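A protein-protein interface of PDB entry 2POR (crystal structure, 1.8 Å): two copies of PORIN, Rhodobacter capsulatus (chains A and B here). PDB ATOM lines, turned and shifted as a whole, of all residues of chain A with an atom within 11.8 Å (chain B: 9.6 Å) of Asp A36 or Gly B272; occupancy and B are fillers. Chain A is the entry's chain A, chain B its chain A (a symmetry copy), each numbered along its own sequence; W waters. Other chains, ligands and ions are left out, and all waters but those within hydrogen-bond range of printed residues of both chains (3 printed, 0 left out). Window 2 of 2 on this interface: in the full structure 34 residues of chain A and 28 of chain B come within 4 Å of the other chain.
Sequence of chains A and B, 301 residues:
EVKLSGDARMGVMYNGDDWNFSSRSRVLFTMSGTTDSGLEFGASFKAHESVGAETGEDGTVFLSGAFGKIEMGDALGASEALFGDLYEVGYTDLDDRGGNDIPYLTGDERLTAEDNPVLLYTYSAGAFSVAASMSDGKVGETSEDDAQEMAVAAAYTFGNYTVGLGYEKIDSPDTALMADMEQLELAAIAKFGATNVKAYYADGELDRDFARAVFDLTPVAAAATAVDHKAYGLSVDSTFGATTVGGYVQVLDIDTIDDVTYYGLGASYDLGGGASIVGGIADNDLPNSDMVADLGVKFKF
Of the 16 printed residues of chain A, 5 touch a printed residue of chain B. Hydrophobic or aromatic side chains of chain A within 4 Å of the printed part of chain B: Phe A41. Among the printed residues, 13 pairs touch across the chains. Among the printed residues, no Asp or Glu carboxylate lies within 4 Å of a Lys or Arg side-chain nitrogen of the other chain.
No position is printed for both chains.
Of the printed residues of chain B, Thr A34 touches Gly B273 (3.3 Å). Asp A36 touches just these residues of chain B: Leu B271 (3.1 Å), Gly B272 (3.6 Å) and Gly B273 (3.98 Å). Ser A37 touches none of the printed residues of chain B. Of the printed residues of chain B, Phe A41 touches Gly B273, Gly B274, Ala B275, Phe B299 and Lys B300. No residue of chain A comes within 4 Å of Asp B270. Leu B271 touches two residues of chain A. Gly B272 touches just these residues of chain A: Thr A35 (3.4 Å) and Asp A36 (3.6 Å). Gly B273 touches three residues of chain A. Of chain A, only Phe A41 (3.9 Å) comes within 4 Å of Gly B274. Printed residues of chain A within 4 Å of Ala B275: Thr A35 and Phe A41. Printed residues of chain A within 4 Å of Lys B300: Phe A41. The nearest residue of chain A that does not touch Gly B272 is Thr A34 (4.1 Å). The nearest printed residue of chain A that does not touch Lys B300 is Glu A1 (5.2 Å).
Thr A34 touches Gly B273 (O to CA, 3.3 Å). CB of Thr A35 touches O of Leu B271, 3.4 Å away. Thr A35 touches Gly B272 (CA to O, 3.4 Å). Thr A35 touches Ala B275. Asp A36 touches Gly B272 (OD1 to CA, 3.6 Å). Asp A36 touches Gly B273. C of Gly B274 touches CZ of Phe A41, 3.9 Å away. Phe A41 touches Ala B275. Phe A41 touches Phe B299 (CD1 to CD1, 3.6 Å). Lys B300 touches Phe A41.
Water W3 lies within hydrogen-bond range of O of Leu B271 (2.6 Å), N of Ser A37 (3.1 Å), OG1 of Thr A35 (3.3 Å) and N of Asp A36 (3.3 Å). Water W1 lies within hydrogen-bond range of O of Gly B273 (2.8 Å) and N of Thr A34 (3.1 Å). Water W2 lies within hydrogen-bond range of the backbone NH of Gly B273 (2.9 Å) and the side-chain carboxylate of Asp A36 (3.2 Å).
The side-chain hydroxyl (OG1) of Thr A34 is in hydrogen-bond range of the side-chain carboxylate (OE1) of Glu A40 (2.8 Å). The backbone NH (N) of Gly B272 is in hydrogen-bond range of the side-chain carboxylate (OD1) of Asp B270, 2.8 Å away. The backbone carbonyl oxygen of Gly A42 lies within hydrogen-bond range of the backbone NH of Phe A62 (2.9 Å). N of Lys B300 is in hydrogen-bond range of O of Gly B274 (2.8 Å). N of Phe A41 lies within hydrogen-bond range of O of Gly A33 (3.0 Å). The backbone NH (N) of Leu A39 lies within hydrogen-bond range of the side-chain hydroxyl (OG1) of Thr A35 (3.1 Å).
N of Asp A36 is in hydrogen-bond range of O of Leu B271, at 3.1 Å.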
ATOM      1  N   GLU A   1     -12.608  27.774  33.465  1.00  0.00           N
ATOM      2  CA  GLU A   1     -11.875  28.725  34.285  1.00  0.00           C
ATOM      3  C   GLU A   1     -10.453  29.045  33.751  1.00  0.00           C
ATOM      4  O   GLU A   1      -9.792  28.097  33.321  1.00  0.00           O
ATOM      5  CB  GLU A   1     -11.815  28.115  35.670  1.00  0.00           C
ATOM      6  CG  GLU A   1     -11.059  28.925  36.714  1.00  0.00           C
ATOM      7  CD  GLU A   1     -10.754  28.173  38.015  1.00  0.00           C
ATOM      8  OE1 GLU A   1     -10.776  26.931  38.034  1.00  0.00           O
ATOM      9  OE2 GLU A   1     -10.480  28.850  39.012  1.00  0.00           O
ATOM     10  N   SER A  32      -8.865  25.334  33.175  1.00  0.00           N
ATOM     11  CA  SER A  32      -9.326  24.052  33.733  1.00  0.00           C
ATOM     12  C   SER A  32     -10.843  23.957  33.825  1.00  0.00           C
ATOM     13  O   SER A  32     -11.531  25.003  33.754  1.00  0.00           O
ATOM     14  CB  SER A  32      -8.717  23.829  35.133  1.00  0.00           C
ATOM     15  OG  SER A  32      -8.873  25.008  35.909  1.00  0.00           O
ATOM     16  N   GLY A  33     -11.286  22.697  33.848  1.00  0.00           N
ATOM     17  CA  GLY A  33     -12.700  22.377  33.910  1.00  0.00           C
ATOM     18  C   GLY A  33     -12.898  20.922  34.336  1.00  0.00           C
ATOM     19  O   GLY A  33     -11.936  20.149  34.433  1.00  0.00           O
ATOM     20  N   THR A  34     -14.166  20.535  34.591  1.00  0.00           N
ATOM     21  CA  THR A  34     -14.540  19.218  35.072  1.00  0.00           C
ATOM     22  C   THR A  34     -15.858  18.889  34.409  1.00  0.00           C
ATOM     23  O   THR A  34     -16.728  19.760  34.340  1.00  0.00           O
ATOM     24  CB  THR A  34     -14.773  19.203  36.602  1.00  0.00           C
ATOM     25  OG1 THR A  34     -13.613  19.732  37.190  1.00  0.00           O
ATOM     26  CG2 THR A  34     -14.926  17.823  37.186  1.00  0.00           C
ATOM     27  N   THR A  35     -16.056  17.675  33.925  1.00  0.00           N
ATOM     28  CA  THR A  35     -17.305  17.359  33.277  1.00  0.00           C
ATOM     29  C   THR A  35     -18.230  16.901  34.421  1.00  0.00           C
ATOM     30  O   THR A  35     -17.791  16.686  35.559  1.00  0.00           O
ATOM     31  CB  THR A  35     -17.084  16.231  32.273  1.00  0.00           C
ATOM     32  OG1 THR A  35     -16.658  15.083  33.022  1.00  0.00           O
ATOM     33  CG2 THR A  35     -16.012  16.604  31.213  1.00  0.00           C
ATOM     34  N   ASP A  36     -19.491  16.634  34.108  1.00  0.00           N
ATOM     35  CA  ASP A  36     -20.503  16.186  35.060  1.00  0.00           C
ATOM     36  C   ASP A  36     -20.073  14.903  35.743  1.00  0.00           C
ATOM     37  O   ASP A  36     -20.280  14.769  36.956  1.00  0.00           O
ATOM     38  CB  ASP A  36     -21.804  16.004  34.302  1.00  0.00           C
ATOM     39  CG  ASP A  36     -22.483  17.317  33.879  1.00  0.00           C
ATOM     40  OD1 ASP A  36     -22.025  18.396  34.310  1.00  0.00           O
ATOM     41  OD2 ASP A  36     -23.460  17.242  33.109  1.00  0.00           O
ATOM     42  N   SER A  37     -19.395  13.961  35.089  1.00  0.00           N
ATOM     43  CA  SER A  37     -18.968  12.773  35.803  1.00  0.00           C
ATOM     44  C   SER A  37     -17.612  12.887  36.479  1.00  0.00           C
ATOM     45  O   SER A  37     -17.123  11.887  37.023  1.00  0.00           O
ATOM     46  CB  SER A  37     -18.982  11.601  34.831  1.00  0.00           C
ATOM     47  OG  SER A  37     -17.987  11.726  33.817  1.00  0.00           O
ATOM     48  N   GLY A  38     -16.964  14.069  36.439  1.00  0.00           N
ATOM     49  CA  GLY A  38     -15.691  14.232  37.103  1.00  0.00           C
ATOM     50  C   GLY A  38     -14.445  13.945  36.254  1.00  0.00           C
ATOM     51  O   GLY A  38     -13.366  13.722  36.825  1.00  0.00           O
ATOM     52  N   LEU A  39     -14.547  13.884  34.914  1.00  0.00           N
ATOM     53  CA  LEU A  39     -13.327  13.856  34.097  1.00  0.00           C
ATOM     54  C   LEU A  39     -12.792  15.286  34.187  1.00  0.00           C
ATOM     55  O   LEU A  39     -13.546  16.267  34.190  1.00  0.00           O
ATOM     56  CB  LEU A  39     -13.614  13.566  32.640  1.00  0.00           C
ATOM     57  CG  LEU A  39     -14.233  12.229  32.371  1.00  0.00           C
ATOM     58  CD1 LEU A  39     -14.458  12.060  30.900  1.00  0.00           C
ATOM     59  CD2 LEU A  39     -13.341  11.180  32.902  1.00  0.00           C
ATOM     60  N   GLU A  40     -11.495  15.494  34.313  1.00  0.00           N
ATOM     61  CA  GLU A  40     -10.924  16.815  34.435  1.00  0.00           C
ATOM     62  C   GLU A  40     -10.311  17.141  33.063  1.00  0.00           C
ATOM     63  O   GLU A  40      -9.809  16.255  32.361  1.00  0.00           O
ATOM     64  CB  GLU A  40      -9.828  16.812  35.472  1.00  0.00           C
ATOM     65  CG  GLU A  40     -10.220  16.361  36.887  1.00  0.00           C
ATOM     66  CD  GLU A  40     -11.204  17.302  37.573  1.00  0.00           C
ATOM     67  OE1 GLU A  40     -11.090  18.519  37.426  1.00  0.00           O
ATOM     68  OE2 GLU A  40     -12.086  16.808  38.269  1.00  0.00           O
ATOM     69  N   PHE A  41     -10.334  18.382  32.651  1.00  0.00           N
ATOM     70  CA  PHE A  41      -9.765  18.760  31.371  1.00  0.00           C
ATOM     71  C   PHE A  41      -9.078  20.089  31.543  1.00  0.00           C
ATOM     72  O   PHE A  41      -9.324  20.804  32.532  1.00  0.00           O
ATOM     73  CB  PHE A  41     -10.885  18.806  30.339  1.00  0.00           C
ATOM     74  CG  PHE A  41     -12.068  19.756  30.545  1.00  0.00           C
ATOM     75  CD1 PHE A  41     -12.024  21.066  30.115  1.00  0.00           C
ATOM     76  CD2 PHE A  41     -13.239  19.260  31.112  1.00  0.00           C
ATOM     77  CE1 PHE A  41     -13.128  21.890  30.230  1.00  0.00           C
ATOM     78  CE2 PHE A  41     -14.345  20.083  31.228  1.00  0.00           C
ATOM     79  CZ  PHE A  41     -14.290  21.388  30.789  1.00  0.00           C
ATOM     80  N   GLY A  42      -8.193  20.463  30.631  1.00  0.00           N
ATOM     81  CA  GLY A  42      -7.518  21.726  30.781  1.00  0.00           C
ATOM     82  C   GLY A  42      -6.634  22.004  29.559  1.00  0.00           C
ATOM     83  O   GLY A  42      -6.622  21.199  28.625  1.00  0.00           O
ATOM     84  N   PHE A  62      -5.410  18.688  27.702  1.00  0.00           N
ATOM     85  CA  PHE A  62      -5.502  17.352  28.285  1.00  0.00           C
ATOM     86  C   PHE A  62      -6.928  17.009  28.736  1.00  0.00           C
ATOM     87  O   PHE A  62      -7.783  17.896  28.915  1.00  0.00           O
ATOM     88  CB  PHE A  62      -4.561  17.218  29.473  1.00  0.00           C
ATOM     89  CG  PHE A  62      -4.998  17.943  30.751  1.00  0.00           C
ATOM     90  CD1 PHE A  62      -5.835  17.304  31.672  1.00  0.00           C
ATOM     91  CD2 PHE A  62      -4.532  19.222  30.994  1.00  0.00           C
ATOM     92  CE1 PHE A  62      -6.194  17.955  32.839  1.00  0.00           C
ATOM     93  CE2 PHE A  62      -4.904  19.860  32.170  1.00  0.00           C
ATOM     94  CZ  PHE A  62      -5.729  19.234  33.093  1.00  0.00           C
ATOM     95  N   LEU A  63      -7.122  15.704  28.890  1.00  0.00           N
ATOM     96  CA  LEU A  63      -8.356  15.098  29.405  1.00  0.00           C
ATOM     97  C   LEU A  63      -7.901  14.010  30.339  1.00  0.00           C
ATOM     98  O   LEU A  63      -7.036  13.238  29.917  1.00  0.00           O
ATOM     99  CB  LEU A  63      -9.208  14.411  28.335  1.00  0.00           C
ATOM    100  CG  LEU A  63     -10.528  13.774  28.799  1.00  0.00           C
ATOM    101  CD1 LEU A  63     -11.506  14.843  29.270  1.00  0.00           C
ATOM    102  CD2 LEU A  63     -11.167  13.079  27.634  1.00  0.00           C
ATOM    103  N   SER A  64      -8.365  13.918  31.603  1.00  0.00           N
ATOM    104  CA  SER A  64      -7.973  12.829  32.496  1.00  0.00           C
ATOM    105  C   SER A  64      -9.186  12.275  33.262  1.00  0.00           C
ATOM    106  O   SER A  64     -10.242  12.890  33.367  1.00  0.00           O
ATOM    107  CB  SER A  64      -6.924  13.283  33.484  1.00  0.00           C
ATOM    108  OG  SER A  64      -7.280  14.420  34.233  1.00  0.00           O
ATOM    109  N   GLY A  65      -9.045  11.048  33.664  1.00  0.00           N
ATOM    110  CA  GLY A  65     -10.087  10.349  34.351  1.00  0.00           C
ATOM    111  C   GLY A  65      -9.430   9.207  35.082  1.00  0.00           C
ATOM    112  O   GLY A  65      -8.215   9.151  35.325  1.00  0.00           O
ATOM    113  N   GLY B 241     -31.559  15.706  24.270  1.00  0.00           N
ATOM    114  CA  GLY B 241     -30.797  15.427  25.461  1.00  0.00           C
ATOM    115  C   GLY B 241     -29.427  16.101  25.396  1.00  0.00           C
ATOM    116  O   GLY B 241     -29.299  17.325  25.257  1.00  0.00           O
ATOM    117  N   ALA B 242     -28.401  15.265  25.523  1.00  0.00           N
ATOM    118  CA  ALA B 242     -27.023  15.720  25.427  1.00  0.00           C
ATOM    119  C   ALA B 242     -26.525  15.711  23.967  1.00  0.00           C
ATOM    120  O   ALA B 242     -25.433  16.220  23.725  1.00  0.00           O
ATOM    121  CB  ALA B 242     -26.161  14.791  26.277  1.00  0.00           C
ATOM    122  N   TYR B 269     -21.884  15.549  21.543  1.00  0.00           N
ATOM    123  CA  TYR B 269     -22.419  15.002  22.743  1.00  0.00           C
ATOM    124  C   TYR B 269     -21.895  15.838  23.886  1.00  0.00           C
ATOM    125  O   TYR B 269     -20.690  15.890  24.138  1.00  0.00           O
ATOM    126  CB  TYR B 269     -21.950  13.589  22.826  1.00  0.00           C
ATOM    127  CG  TYR B 269     -22.567  12.943  24.035  1.00  0.00           C
ATOM    128  CD1 TYR B 269     -23.859  12.461  23.957  1.00  0.00           C
ATOM    129  CD2 TYR B 269     -21.859  12.908  25.215  1.00  0.00           C
ATOM    130  CE1 TYR B 269     -24.452  11.941  25.092  1.00  0.00           C
ATOM    131  CE2 TYR B 269     -22.448  12.397  26.351  1.00  0.00           C
ATOM    132  CZ  TYR B 269     -23.743  11.915  26.282  1.00  0.00           C
ATOM    133  OH  TYR B 269     -24.331  11.403  27.430  1.00  0.00           O
ATOM    134  N   ASP B 270     -22.764  16.466  24.642  1.00  0.00           N
ATOM    135  CA  ASP B 270     -22.336  17.308  25.737  1.00  0.00           C
ATOM    136  C   ASP B 270     -21.975  16.492  26.985  1.00  0.00           C
ATOM    137  O   ASP B 270     -22.804  15.729  27.481  1.00  0.00           O
ATOM    138  CB  ASP B 270     -23.481  18.293  25.994  1.00  0.00           C
ATOM    139  CG  ASP B 270     -23.190  19.455  26.936  1.00  0.00           C
ATOM    140  OD1 ASP B 270     -22.160  19.437  27.599  1.00  0.00           O
ATOM    141  OD2 ASP B 270     -23.983  20.399  26.992  1.00  0.00           O
ATOM    142  N   LEU B 271     -20.765  16.620  27.516  1.00  0.00           N
ATOM    143  CA  LEU B 271     -20.329  15.940  28.726  1.00  0.00           C
ATOM    144  C   LEU B 271     -20.572  16.823  29.958  1.00  0.00           C
ATOM    145  O   LEU B 271     -20.273  16.427  31.074  1.00  0.00           O
ATOM    146  CB  LEU B 271     -18.842  15.640  28.687  1.00  0.00           C
ATOM    147  CG  LEU B 271     -18.277  14.774  27.560  1.00  0.00           C
ATOM    148  CD1 LEU B 271     -16.768  14.645  27.692  1.00  0.00           C
ATOM    149  CD2 LEU B 271     -18.905  13.430  27.620  1.00  0.00           C
ATOM    150  N   GLY B 272     -20.993  18.054  29.772  1.00  0.00           N
ATOM    151  CA  GLY B 272     -21.192  19.018  30.814  1.00  0.00           C
ATOM    152  C   GLY B 272     -19.912  19.722  31.221  1.00  0.00           C
ATOM    153  O   GLY B 272     -18.811  19.294  30.879  1.00  0.00           O
ATOM    154  N   GLY B 273     -20.000  20.854  31.923  1.00  0.00           N
ATOM    155  CA  GLY B 273     -18.835  21.477  32.501  1.00  0.00           C
ATOM    156  C   GLY B 273     -18.023  22.263  31.468  1.00  0.00           C
ATOM    157  O   GLY B 273     -17.025  22.870  31.833  1.00  0.00           O
ATOM    158  N   GLY B 274     -18.468  22.333  30.206  1.00  0.00           N
ATOM    159  CA  GLY B 274     -17.770  23.041  29.130  1.00  0.00           C
ATOM    160  C   GLY B 274     -17.090  22.063  28.155  1.00  0.00           C
ATOM    161  O   GLY B 274     -16.315  22.522  27.323  1.00  0.00           O
ATOM    162  N   ALA B 275     -17.327  20.752  28.222  1.00  0.00           N
ATOM    163  CA  ALA B 275     -16.683  19.778  27.368  1.00  0.00           C
ATOM    164  C   ALA B 275     -17.707  19.027  26.549  1.00  0.00           C
ATOM    165  O   ALA B 275     -18.824  18.776  27.012  1.00  0.00           O
ATOM    166  CB  ALA B 275     -15.897  18.776  28.200  1.00  0.00           C
ATOM    167  N   SER B 276     -17.377  18.699  25.298  1.00  0.00           N
ATOM    168  CA  SER B 276     -18.234  17.925  24.427  1.00  0.00           C
ATOM    169  C   SER B 276     -17.377  17.064  23.484  1.00  0.00           C
ATOM    170  O   SER B 276     -16.205  17.389  23.233  1.00  0.00           O
ATOM    171  CB  SER B 276     -19.162  18.870  23.631  1.00  0.00           C
ATOM    172  OG  SER B 276     -18.519  19.988  23.041  1.00  0.00           O
ATOM    173  N   ILE B 277     -17.887  15.921  23.050  1.00  0.00           N
ATOM    174  CA  ILE B 277     -17.225  15.045  22.096  1.00  0.00           C
ATOM    175  C   ILE B 277     -17.880  15.465  20.794  1.00  0.00           C
ATOM    176  O   ILE B 277     -19.117  15.580  20.737  1.00  0.00           O
ATOM    177  CB  ILE B 277     -17.531  13.584  22.446  1.00  0.00           C
ATOM    178  CG1 ILE B 277     -16.904  13.231  23.754  1.00  0.00           C
ATOM    179  CG2 ILE B 277     -16.963  12.643  21.382  1.00  0.00           C
ATOM    180  CD1 ILE B 277     -17.440  11.867  24.229  1.00  0.00           C
ATOM    181  N   LYS B 298     -14.036  19.205  22.393  1.00  0.00           N
ATOM    182  CA  LYS B 298     -13.905  20.656  22.391  1.00  0.00           C
ATOM    183  C   LYS B 298     -14.120  21.110  23.829  1.00  0.00           C
ATOM    184  O   LYS B 298     -14.954  20.505  24.507  1.00  0.00           O
ATOM    185  CB  LYS B 298     -14.959  21.305  21.530  1.00  0.00           C
ATOM    186  CG  LYS B 298     -14.635  21.146  20.058  1.00  0.00           C
ATOM    187  CD  LYS B 298     -15.808  21.605  19.285  1.00  0.00           C
ATOM    188  CE  LYS B 298     -15.853  23.075  19.401  1.00  0.00           C
ATOM    189  NZ  LYS B 298     -16.986  23.562  18.637  1.00  0.00           N
ATOM    190  N   PHE B 299     -13.406  22.104  24.338  1.00  0.00           N
ATOM    191  CA  PHE B 299     -13.483  22.551  25.723  1.00  0.00           C
ATOM    192  C   PHE B 299     -13.707  24.039  25.743  1.00  0.00           C
ATOM    193  O   PHE B 299     -13.186  24.767  24.882  1.00  0.00           O
ATOM    194  CB  PHE B 299     -12.185  22.259  26.425  1.00  0.00           C
ATOM    195  CG  PHE B 299     -11.750  20.810  26.482  1.00  0.00           C
ATOM    196  CD1 PHE B 299     -12.635  19.802  26.821  1.00  0.00           C
ATOM    197  CD2 PHE B 299     -10.438  20.491  26.223  1.00  0.00           C
ATOM    198  CE1 PHE B 299     -12.213  18.490  26.906  1.00  0.00           C
ATOM    199  CE2 PHE B 299     -10.032  19.173  26.317  1.00  0.00           C
ATOM    200  CZ  PHE B 299     -10.908  18.169  26.656  1.00  0.00           C
ATOM    201  N   LYS B 300     -14.482  24.568  26.662  1.00  0.00           N
ATOM    202  CA  LYS B 300     -14.644  26.005  26.816  1.00  0.00           C
ATOM    203  C   LYS B 300     -14.208  26.308  28.245  1.00  0.00           C
ATOM    204  O   LYS B 300     -14.412  25.463  29.149  1.00  0.00           O
ATOM    205  CB  LYS B 300     -16.074  26.395  26.647  1.00  0.00           C
ATOM    206  CG  LYS B 300     -16.568  26.168  25.260  1.00  0.00           C
ATOM    207  CD  LYS B 300     -17.696  27.143  24.919  1.00  0.00           C
ATOM    208  CE  LYS B 300     -19.045  26.841  25.574  1.00  0.00           C
ATOM    209  NZ  LYS B 300     -20.061  27.781  25.110  1.00  0.00           N
HETATM  210  O   HOH W   1     -15.982  23.017  34.383  1.00  0.00           O
HETATM  211  O   HOH W   2     -22.650  21.297  33.083  1.00  0.00           O
HETATM  212  O   HOH W   3     -19.605  14.047  32.014  1.00  0.00           O
